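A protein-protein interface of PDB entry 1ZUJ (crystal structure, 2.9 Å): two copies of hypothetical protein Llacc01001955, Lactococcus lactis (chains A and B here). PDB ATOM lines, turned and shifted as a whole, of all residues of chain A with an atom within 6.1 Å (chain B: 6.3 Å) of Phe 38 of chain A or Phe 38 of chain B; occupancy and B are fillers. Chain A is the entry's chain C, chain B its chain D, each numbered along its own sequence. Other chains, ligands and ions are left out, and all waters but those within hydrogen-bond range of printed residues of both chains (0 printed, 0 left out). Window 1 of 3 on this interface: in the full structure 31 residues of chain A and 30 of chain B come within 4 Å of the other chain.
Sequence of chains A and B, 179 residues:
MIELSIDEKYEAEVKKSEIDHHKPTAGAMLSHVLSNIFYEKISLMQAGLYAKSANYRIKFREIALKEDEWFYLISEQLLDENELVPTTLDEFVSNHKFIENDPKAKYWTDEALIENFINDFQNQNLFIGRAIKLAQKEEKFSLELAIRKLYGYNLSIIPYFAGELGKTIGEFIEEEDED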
ATOM      1  N   VAL A  33     -26.411  23.725  16.919  1.00  0.00           N
ATOM      2  CA  VAL A  33     -25.937  22.461  17.482  1.00  0.00           C
ATOM      3  C   VAL A  33     -25.130  21.651  16.477  1.00  0.00           C
ATOM      4  O   VAL A  33     -24.051  21.170  16.773  1.00  0.00           O
ATOM      5  CB  VAL A  33     -27.108  21.592  17.939  1.00  0.00           C
ATOM      6  CG1 VAL A  33     -26.621  20.200  18.350  1.00  0.00           C
ATOM      7  CG2 VAL A  33     -27.858  22.281  19.086  1.00  0.00           C
ATOM      8  N   LEU A  34     -25.690  21.494  15.295  1.00  0.00           N
ATOM      9  CA  LEU A  34     -25.075  20.742  14.236  1.00  0.00           C
ATOM     10  C   LEU A  34     -23.866  21.487  13.714  1.00  0.00           C
ATOM     11  O   LEU A  34     -22.911  20.875  13.280  1.00  0.00           O
ATOM     12  CB  LEU A  34     -26.081  20.519  13.112  1.00  0.00           C
ATOM     13  CG  LEU A  34     -27.294  19.667  13.513  1.00  0.00           C
ATOM     14  CD1 LEU A  34     -28.445  19.837  12.530  1.00  0.00           C
ATOM     15  CD2 LEU A  34     -26.913  18.199  13.648  1.00  0.00           C
ATOM     16  N   SER A  35     -23.888  22.808  13.755  1.00  0.00           N
ATOM     17  CA  SER A  35     -22.808  23.577  13.152  1.00  0.00           C
ATOM     18  C   SER A  35     -21.598  23.496  14.061  1.00  0.00           C
ATOM     19  O   SER A  35     -20.457  23.634  13.637  1.00  0.00           O
ATOM     20  CB  SER A  35     -23.230  25.040  12.924  1.00  0.00           C
ATOM     21  OG  SER A  35     -24.034  25.165  11.766  1.00  0.00           O
ATOM     22  N   ASN A  36     -21.868  23.257  15.332  1.00  0.00           N
ATOM     23  CA  ASN A  36     -20.821  23.190  16.353  1.00  0.00           C
ATOM     24  C   ASN A  36     -20.260  21.788  16.460  1.00  0.00           C
ATOM     25  O   ASN A  36     -19.065  21.618  16.735  1.00  0.00           O
ATOM     26  CB  ASN A  36     -21.383  23.626  17.707  1.00  0.00           C
ATOM     27  CG  ASN A  36     -21.497  25.127  17.830  1.00  0.00           C
ATOM     28  OD1 ASN A  36     -21.781  25.615  18.891  1.00  0.00           O
ATOM     29  ND2 ASN A  36     -21.278  25.857  16.745  1.00  0.00           N
ATOM     30  N   ILE A  37     -21.129  20.795  16.252  1.00  0.00           N
ATOM     31  CA  ILE A  37     -20.689  19.432  16.108  1.00  0.00           C
ATOM     32  C   ILE A  37     -19.683  19.366  14.951  1.00  0.00           C
ATOM     33  O   ILE A  37     -18.660  18.687  15.031  1.00  0.00           O
ATOM     34  CB  ILE A  37     -21.891  18.520  15.907  1.00  0.00           C
ATOM     35  CG1 ILE A  37     -22.352  18.001  17.263  1.00  0.00           C
ATOM     36  CG2 ILE A  37     -21.552  17.340  15.053  1.00  0.00           C
ATOM     37  CD1 ILE A  37     -23.758  17.467  17.250  1.00  0.00           C
ATOM     38  N   PHE A  38     -19.955  20.122  13.902  1.00  0.00           N
ATOM     39  CA  PHE A  38     -19.072  20.179  12.762  1.00  0.00           C
ATOM     40  C   PHE A  38     -17.726  20.761  13.188  1.00  0.00           C
ATOM     41  O   PHE A  38     -16.673  20.152  13.047  1.00  0.00           O
ATOM     42  CB  PHE A  38     -19.705  21.045  11.690  1.00  0.00           C
ATOM     43  CG  PHE A  38     -18.853  21.230  10.482  1.00  0.00           C
ATOM     44  CD1 PHE A  38     -18.262  22.454  10.217  1.00  0.00           C
ATOM     45  CD2 PHE A  38     -18.648  20.192   9.605  1.00  0.00           C
ATOM     46  CE1 PHE A  38     -17.475  22.632   9.096  1.00  0.00           C
ATOM     47  CE2 PHE A  38     -17.858  20.367   8.474  1.00  0.00           C
ATOM     48  CZ  PHE A  38     -17.269  21.585   8.221  1.00  0.00           C
ATOM     49  N   TYR A  39     -17.749  21.951  13.739  1.00  0.00           N
ATOM     50  CA  TYR A  39     -16.501  22.535  14.184  1.00  0.00           C
ATOM     51  C   TYR A  39     -15.781  21.603  15.148  1.00  0.00           C
ATOM     52  O   TYR A  39     -14.555  21.593  15.183  1.00  0.00           O
ATOM     53  CB  TYR A  39     -16.737  23.920  14.830  1.00  0.00           C
ATOM     54  CG  TYR A  39     -16.623  25.076  13.845  1.00  0.00           C
ATOM     55  CD1 TYR A  39     -15.564  25.942  13.895  1.00  0.00           C
ATOM     56  CD2 TYR A  39     -17.582  25.281  12.866  1.00  0.00           C
ATOM     57  CE1 TYR A  39     -15.456  26.974  13.002  1.00  0.00           C
ATOM     58  CE2 TYR A  39     -17.488  26.328  11.973  1.00  0.00           C
ATOM     59  CZ  TYR A  39     -16.417  27.158  12.041  1.00  0.00           C
ATOM     60  OH  TYR A  39     -16.302  28.198  11.164  1.00  0.00           O
ATOM     61  N   GLU A  40     -16.537  20.825  15.921  1.00  0.00           N
ATOM     62  CA  GLU A  40     -15.935  20.033  16.998  1.00  0.00           C
ATOM     63  C   GLU A  40     -15.100  18.930  16.370  1.00  0.00           C
ATOM     64  O   GLU A  40     -13.906  18.862  16.606  1.00  0.00           O
ATOM     65  CB  GLU A  40     -16.981  19.477  17.978  1.00  0.00           C
ATOM     66  CG  GLU A  40     -16.378  18.999  19.294  1.00  0.00           C
ATOM     67  CD  GLU A  40     -15.815  20.127  20.159  1.00  0.00           C
ATOM     68  OE1 GLU A  40     -16.602  20.872  20.777  1.00  0.00           O
ATOM     69  OE2 GLU A  40     -14.573  20.262  20.259  1.00  0.00           O
ATOM     70  N   LYS A  41     -15.746  18.114  15.539  1.00  0.00           N
ATOM     71  CA  LYS A  41     -15.089  17.149  14.678  1.00  0.00           C
ATOM     72  C   LYS A  41     -13.744  17.711  14.274  1.00  0.00           C
ATOM     73  O   LYS A  41     -12.753  17.047  14.418  1.00  0.00           O
ATOM     74  CB  LYS A  41     -15.953  16.865  13.430  1.00  0.00           C
ATOM     75  CG  LYS A  41     -16.095  15.389  12.963  1.00  0.00           C
ATOM     76  CD  LYS A  41     -15.083  14.973  11.781  1.00  0.00           C
ATOM     77  CE  LYS A  41     -15.290  15.747  10.392  1.00  0.00           C
ATOM     78  NZ  LYS A  41     -14.049  15.978   9.507  1.00  0.00           N
ATOM     79  N   ILE A  42     -13.681  18.940  13.790  1.00  0.00           N
ATOM     80  CA  ILE A  42     -12.408  19.431  13.276  1.00  0.00           C
ATOM     81  C   ILE A  42     -11.329  19.487  14.323  1.00  0.00           C
ATOM     82  O   ILE A  42     -10.198  19.160  14.035  1.00  0.00           O
ATOM     83  CB  ILE A  42     -12.501  20.804  12.602  1.00  0.00           C
ATOM     84  CG1 ILE A  42     -13.329  20.734  11.322  1.00  0.00           C
ATOM     85  CG2 ILE A  42     -11.101  21.288  12.232  1.00  0.00           C
ATOM     86  CD1 ILE A  42     -13.788  22.124  10.825  1.00  0.00           C
ATOM     87  N   SER A  43     -11.651  19.956  15.517  1.00  0.00           N
ATOM     88  CA  SER A  43     -10.632  20.124  16.551  1.00  0.00           C
ATOM     89  C   SER A  43     -10.267  18.772  17.081  1.00  0.00           C
ATOM     90  O   SER A  43      -9.120  18.513  17.385  1.00  0.00           O
ATOM     91  CB  SER A  43     -11.134  21.004  17.703  1.00  0.00           C
ATOM     92  OG  SER A  43     -11.224  22.381  17.326  1.00  0.00           O
ATOM     93  N   MET A  45     -10.271  15.948  15.501  1.00  0.00           N
ATOM     94  CA  MET A  45      -9.434  15.270  14.509  1.00  0.00           C
ATOM     95  C   MET A  45      -8.014  15.751  14.720  1.00  0.00           C
ATOM     96  O   MET A  45      -7.071  14.967  14.765  1.00  0.00           O
ATOM     97  CB  MET A  45      -9.889  15.623  13.081  1.00  0.00           C
ATOM     98  CG  MET A  45      -9.923  14.446  12.101  1.00  0.00           C
ATOM     99  SD  MET A  45     -11.592  14.141  11.284  1.00  0.00           S
ATOM    100  CE  MET A  45     -11.070  13.880   9.535  1.00  0.00           C
ATOM    101  N   PHE A  71     -24.348  13.905  14.389  1.00  0.00           N
ATOM    102  CA  PHE A  71     -24.684  14.840  13.333  1.00  0.00           C
ATOM    103  C   PHE A  71     -25.677  14.218  12.362  1.00  0.00           C
ATOM    104  O   PHE A  71     -26.596  14.893  11.914  1.00  0.00           O
ATOM    105  CB  PHE A  71     -23.435  15.285  12.583  1.00  0.00           C
ATOM    106  CG  PHE A  71     -23.697  16.300  11.482  1.00  0.00           C
ATOM    107  CD1 PHE A  71     -23.259  17.616  11.609  1.00  0.00           C
ATOM    108  CD2 PHE A  71     -24.348  15.937  10.307  1.00  0.00           C
ATOM    109  CE1 PHE A  71     -23.474  18.528  10.595  1.00  0.00           C
ATOM    110  CE2 PHE A  71     -24.551  16.861   9.304  1.00  0.00           C
ATOM    111  CZ  PHE A  71     -24.131  18.143   9.450  1.00  0.00           C
ATOM    112  N   LEU A  89     -20.352  24.655   4.153  1.00  0.00           N
ATOM    113  CA  LEU A  89     -19.424  25.529   4.915  1.00  0.00           C
ATOM    114  C   LEU A  89     -20.002  26.893   5.338  1.00  0.00           C
ATOM    115  O   LEU A  89     -19.718  27.368   6.434  1.00  0.00           O
ATOM    116  CB  LEU A  89     -18.102  25.756   4.153  1.00  0.00           C
ATOM    117  CG  LEU A  89     -16.813  25.146   4.723  1.00  0.00           C
ATOM    118  CD1 LEU A  89     -15.601  25.639   3.936  1.00  0.00           C
ATOM    119  CD2 LEU A  89     -16.582  25.416   6.198  1.00  0.00           C
ATOM    120  N   PHE A  92     -22.463  26.470   8.211  1.00  0.00           N
ATOM    121  CA  PHE A  92     -21.756  26.090   9.432  1.00  0.00           C
ATOM    122  C   PHE A  92     -20.860  27.204  10.062  1.00  0.00           C
ATOM    123  O   PHE A  92     -20.428  27.046  11.205  1.00  0.00           O
ATOM    124  CB  PHE A  92     -20.858  24.867   9.166  1.00  0.00           C
ATOM    125  CG  PHE A  92     -21.583  23.597   8.780  1.00  0.00           C
ATOM    126  CD1 PHE A  92     -20.991  22.715   7.887  1.00  0.00           C
ATOM    127  CD2 PHE A  92     -22.783  23.240   9.339  1.00  0.00           C
ATOM    128  CE1 PHE A  92     -21.598  21.534   7.542  1.00  0.00           C
ATOM    129  CE2 PHE A  92     -23.400  22.048   8.984  1.00  0.00           C
ATOM    130  CZ  PHE A  92     -22.802  21.204   8.089  1.00  0.00           C
ATOM    131  N   VAL B  33      -4.455  17.791  -1.330  1.00  0.00           N
ATOM    132  CA  VAL B  33      -5.169  16.536  -1.472  1.00  0.00           C
ATOM    133  C   VAL B  33      -6.119  16.421  -0.304  1.00  0.00           C
ATOM    134  O   VAL B  33      -7.330  16.272  -0.486  1.00  0.00           O
ATOM    135  CB  VAL B  33      -4.215  15.369  -1.631  1.00  0.00           C
ATOM    136  CG1 VAL B  33      -4.889  14.028  -1.336  1.00  0.00           C
ATOM    137  CG2 VAL B  33      -3.644  15.400  -3.062  1.00  0.00           C
ATOM    138  N   LEU B  34      -5.578  16.632   0.883  1.00  0.00           N
ATOM    139  CA  LEU B  34      -6.306  16.433   2.131  1.00  0.00           C
ATOM    140  C   LEU B  34      -7.428  17.440   2.317  1.00  0.00           C
ATOM    141  O   LEU B  34      -8.504  17.107   2.778  1.00  0.00           O
ATOM    142  CB  LEU B  34      -5.317  16.529   3.289  1.00  0.00           C
ATOM    143  CG  LEU B  34      -4.456  15.289   3.496  1.00  0.00           C
ATOM    144  CD1 LEU B  34      -3.215  15.620   4.260  1.00  0.00           C
ATOM    145  CD2 LEU B  34      -5.263  14.277   4.248  1.00  0.00           C
ATOM    146  N   SER B  35      -7.145  18.681   1.947  1.00  0.00           N
ATOM    147  CA  SER B  35      -8.142  19.762   1.926  1.00  0.00           C
ATOM    148  C   SER B  35      -9.324  19.425   1.052  1.00  0.00           C
ATOM    149  O   SER B  35     -10.471  19.626   1.455  1.00  0.00           O
ATOM    150  CB  SER B  35      -7.502  21.044   1.432  1.00  0.00           C
ATOM    151  OG  SER B  35      -6.499  21.452   2.335  1.00  0.00           O
ATOM    152  N   ASN B  36      -9.055  18.869  -0.129  1.00  0.00           N
ATOM    153  CA  ASN B  36     -10.140  18.416  -0.985  1.00  0.00           C
ATOM    154  C   ASN B  36     -10.901  17.232  -0.430  1.00  0.00           C
ATOM    155  O   ASN B  36     -12.094  17.151  -0.612  1.00  0.00           O
ATOM    156  CB  ASN B  36      -9.644  18.079  -2.361  1.00  0.00           C
ATOM    157  CG  ASN B  36      -9.077  19.271  -3.076  1.00  0.00           C
ATOM    158  OD1 ASN B  36      -9.799  20.104  -3.607  1.00  0.00           O
ATOM    159  ND2 ASN B  36      -7.768  19.347  -3.106  1.00  0.00           N
ATOM    160  N   ILE B  37     -10.251  16.309   0.261  1.00  0.00           N
ATOM    161  CA  ILE B  37     -11.026  15.259   0.941  1.00  0.00           C
ATOM    162  C   ILE B  37     -11.998  15.908   1.943  1.00  0.00           C
ATOM    163  O   ILE B  37     -13.154  15.520   2.051  1.00  0.00           O
ATOM    164  CB  ILE B  37     -10.106  14.298   1.660  1.00  0.00           C
ATOM    165  CG1 ILE B  37      -9.037  13.819   0.686  1.00  0.00           C
ATOM    166  CG2 ILE B  37     -10.903  13.175   2.221  1.00  0.00           C
ATOM    167  CD1 ILE B  37      -8.618  12.375   0.819  1.00  0.00           C
ATOM    168  N   PHE B  38     -11.498  16.913   2.655  1.00  0.00           N
ATOM    169  CA  PHE B  38     -12.269  17.594   3.667  1.00  0.00           C
ATOM    170  C   PHE B  38     -13.478  18.326   3.062  1.00  0.00           C
ATOM    171  O   PHE B  38     -14.569  18.423   3.672  1.00  0.00           O
ATOM    172  CB  PHE B  38     -11.414  18.598   4.429  1.00  0.00           C
ATOM    173  CG  PHE B  38     -12.218  19.439   5.332  1.00  0.00           C
ATOM    174  CD1 PHE B  38     -12.687  20.669   4.908  1.00  0.00           C
ATOM    175  CD2 PHE B  38     -12.608  18.947   6.560  1.00  0.00           C
ATOM    176  CE1 PHE B  38     -13.495  21.428   5.739  1.00  0.00           C
ATOM    177  CE2 PHE B  38     -13.399  19.682   7.399  1.00  0.00           C
ATOM    178  CZ  PHE B  38     -13.854  20.927   6.999  1.00  0.00           C
ATOM    179  N   TYR B  39     -13.277  18.845   1.865  1.00  0.00           N
ATOM    180  CA  TYR B  39     -14.369  19.476   1.211  1.00  0.00           C
ATOM    181  C   TYR B  39     -15.313  18.349   0.740  1.00  0.00           C
ATOM    182  O   TYR B  39     -16.471  18.329   1.108  1.00  0.00           O
ATOM    183  CB  TYR B  39     -13.858  20.408   0.113  1.00  0.00           C
ATOM    184  CG  TYR B  39     -13.677  21.881   0.534  1.00  0.00           C
ATOM    185  CD1 TYR B  39     -14.473  22.871  -0.014  1.00  0.00           C
ATOM    186  CD2 TYR B  39     -12.699  22.283   1.473  1.00  0.00           C
ATOM    187  CE1 TYR B  39     -14.324  24.204   0.342  1.00  0.00           C
ATOM    188  CE2 TYR B  39     -12.542  23.627   1.835  1.00  0.00           C
ATOM    189  CZ  TYR B  39     -13.375  24.581   1.263  1.00  0.00           C
ATOM    190  OH  TYR B  39     -13.270  25.937   1.547  1.00  0.00           O
ATOM    191  N   GLU B  40     -14.809  17.387  -0.022  1.00  0.00           N
ATOM    192  CA  GLU B  40     -15.603  16.240  -0.485  1.00  0.00           C
ATOM    193  C   GLU B  40     -16.521  15.670   0.594  1.00  0.00           C
ATOM    194  O   GLU B  40     -17.673  15.400   0.330  1.00  0.00           O
ATOM    195  CB  GLU B  40     -14.694  15.092  -0.977  1.00  0.00           C
ATOM    196  CG  GLU B  40     -14.450  15.011  -2.481  1.00  0.00           C
ATOM    197  CD  GLU B  40     -15.718  15.133  -3.306  1.00  0.00           C
ATOM    198  OE1 GLU B  40     -15.717  15.848  -4.305  1.00  0.00           O
ATOM    199  OE2 GLU B  40     -16.732  14.513  -2.953  1.00  0.00           O
ATOM    200  N   LYS B  41     -15.990  15.476   1.799  1.00  0.00           N
ATOM    201  CA  LYS B  41     -16.730  14.901   2.916  1.00  0.00           C
ATOM    202  C   LYS B  41     -18.074  15.646   3.103  1.00  0.00           C
ATOM    203  O   LYS B  41     -19.135  15.025   3.359  1.00  0.00           O
ATOM    204  CB  LYS B  41     -15.864  14.948   4.200  1.00  0.00           C
ATOM    205  CG  LYS B  41     -15.812  13.651   5.059  1.00  0.00           C
ATOM    206  CD  LYS B  41     -15.449  13.913   6.578  1.00  0.00           C
ATOM    207  CE  LYS B  41     -16.297  13.001   7.580  1.00  0.00           C
ATOM    208  NZ  LYS B  41     -15.884  13.017   9.046  1.00  0.00           N
ATOM    209  N   ILE B  42     -18.035  16.962   2.933  1.00  0.00           N
ATOM    210  CA  ILE B  42     -19.215  17.796   3.099  1.00  0.00           C
ATOM    211  C   ILE B  42     -20.220  17.616   1.983  1.00  0.00           C
ATOM    212  O   ILE B  42     -21.379  17.411   2.293  1.00  0.00           O
ATOM    213  CB  ILE B  42     -18.868  19.294   3.157  1.00  0.00           C
ATOM    214  CG1 ILE B  42     -17.960  19.638   4.326  1.00  0.00           C
ATOM    215  CG2 ILE B  42     -20.136  20.125   3.241  1.00  0.00           C
ATOM    216  CD1 ILE B  42     -17.130  20.847   4.036  1.00  0.00           C
ATOM    217  N   SER B  43     -19.811  17.763   0.709  1.00  0.00           N
ATOM    218  CA  SER B  43     -20.753  17.634  -0.433  1.00  0.00           C
ATOM    219  C   SER B  43     -21.419  16.249  -0.435  1.00  0.00           C
ATOM    220  O   SER B  43     -22.583  16.082  -0.822  1.00  0.00           O
ATOM    221  CB  SER B  43     -20.049  17.812  -1.782  1.00  0.00           C
ATOM    222  OG  SER B  43     -19.675  19.154  -2.075  1.00  0.00           O
ATOM    223  N   GLU B  67     -13.721   8.692   3.009  1.00  0.00           N
ATOM    224  CA  GLU B  67     -12.854   9.856   2.817  1.00  0.00           C
ATOM    225  C   GLU B  67     -12.192  10.266   4.132  1.00  0.00           C
ATOM    226  O   GLU B  67     -11.029  10.575   4.218  1.00  0.00           O
ATOM    227  CB  GLU B  67     -13.663  11.044   2.283  1.00  0.00           C
ATOM    228  CG  GLU B  67     -14.170  10.864   0.882  1.00  0.00           C
ATOM    229  CD  GLU B  67     -13.156  11.199  -0.169  1.00  0.00           C
ATOM    230  OE1 GLU B  67     -13.351  12.231  -0.807  1.00  0.00           O
ATOM    231  OE2 GLU B  67     -12.202  10.431  -0.408  1.00  0.00           O
ATOM    232  N   PHE B  71      -8.464  10.238   5.078  1.00  0.00           N
ATOM    233  CA  PHE B  71      -7.888  11.439   5.654  1.00  0.00           C
ATOM    234  C   PHE B  71      -6.915  11.029   6.704  1.00  0.00           C
ATOM    235  O   PHE B  71      -5.765  11.417   6.639  1.00  0.00           O
ATOM    236  CB  PHE B  71      -8.947  12.364   6.278  1.00  0.00           C
ATOM    237  CG  PHE B  71      -8.405  13.703   6.664  1.00  0.00           C
ATOM    238  CD1 PHE B  71      -8.285  14.704   5.722  1.00  0.00           C
ATOM    239  CD2 PHE B  71      -7.939  13.932   7.954  1.00  0.00           C
ATOM    240  CE1 PHE B  71      -7.735  15.924   6.059  1.00  0.00           C
ATOM    241  CE2 PHE B  71      -7.403  15.154   8.292  1.00  0.00           C
ATOM    242  CZ  PHE B  71      -7.301  16.156   7.330  1.00  0.00           C
ATOM    243  N   LEU B  89      -9.777  24.581   9.767  1.00  0.00           N
ATOM    244  CA  LEU B  89     -10.600  25.170   8.695  1.00  0.00           C
ATOM    245  C   LEU B  89      -9.871  26.194   7.838  1.00  0.00           C
ATOM    246  O   LEU B  89     -10.077  26.264   6.640  1.00  0.00           O
ATOM    247  CB  LEU B  89     -11.856  25.849   9.252  1.00  0.00           C
ATOM    248  CG  LEU B  89     -13.123  25.551   8.438  1.00  0.00           C
ATOM    249  CD1 LEU B  89     -14.385  26.137   9.076  1.00  0.00           C
ATOM    250  CD2 LEU B  89     -12.972  26.049   7.012  1.00  0.00           C
ATOM    251  N   PHE B  92      -7.685  24.467   5.390  1.00  0.00           N
ATOM    252  CA  PHE B  92      -8.511  23.759   4.398  1.00  0.00           C
ATOM    253  C   PHE B  92      -9.063  24.687   3.335  1.00  0.00           C
ATOM    254  O   PHE B  92      -9.296  24.277   2.217  1.00  0.00           O
ATOM    255  CB  PHE B  92      -9.698  23.020   5.060  1.00  0.00           C
ATOM    256  CG  PHE B  92      -9.293  21.893   5.976  1.00  0.00           C
ATOM    257  CD1 PHE B  92     -10.085  21.548   7.034  1.00  0.00           C
ATOM    258  CD2 PHE B  92      -8.113  21.179   5.783  1.00  0.00           C
ATOM    259  CE1 PHE B  92      -9.714  20.547   7.880  1.00  0.00           C
ATOM    260  CE2 PHE B  92      -7.745  20.165   6.636  1.00  0.00           C
ATOM    261  CZ  PHE B  92      -8.541  19.854   7.682  1.00  0.00           C
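The side-chain amino group (NZ) of Lys 41 of chain A lies within hydrogen-bond range of the side-chain sulfur (SD) of Met 45 of chain A (3.5 Å).
Phe 38 of chain A touches Phe 38 of chain B. OH of Tyr 39 of chain A touches CD1 of Leu 89 of chain B, 3.5 Å away. CE of Lys 41 of chain A touches NZ of Lys 41 of chain B (3.1 Å). Met 45 of chain A touches Phe 71 of chain B (CE to CD2, 3.5 Å). OH of Tyr 39 of chain B touches CD1 of Leu 89 of chain A, at 3.4 Å. CD2 of Leu 89 of chain A touches CD1 of Leu 89 of chain B, at 3.7 Å.
Of chain B, only Phe 38 comes within 4 Å of Phe 38 of chain A. Of the printed residues of chain A, Phe 38 of chain B touches Phe 38. Printed residues of chain B within 4 Å of Met 45 of chain A: Phe 71. Of the printed residues of chain A, Leu 89 of chain B touches Tyr 39 and Leu 89. Of the printed residues of chain B, Leu 89 of chain A touches Tyr 39 (3.4 Å) and Leu 89 (3.7 Å). Printed residues of chain A within 4 Å of Tyr 39 of chain B: Leu 89 (3.4 Å). Phe 92 of chain B touches none of the printed residues of chain A. Ser 43 of chain A touches none of the printed residues of chain B. The nearest residue of chain B that does not touch Phe 38 of chain A is Ile 42 of chain B (4.2 Å). The nearest printed residue of chain A that does not touch Leu 89 of chain B is Ile 42 of chain A (4.2 Å).
Of the 15 printed residues of chain B, 5 touch a printed residue of chain A. Along chain B the printed residues that touch a printed residue of chain A span positions 38 to 89.
Phe 38 of chain B touches its own counterpart, Phe 38 of chain A. Tyr 39 of chain A touches Leu 89 of chain B, and with the chains exchanged Leu 89 of chain A touches Tyr 39 of chain B. Lys 41 of chain B touches its own counterpart, Lys 41 of chain A. Leu 89 of chain A touches its own counterpart, Leu 89 of chain B.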
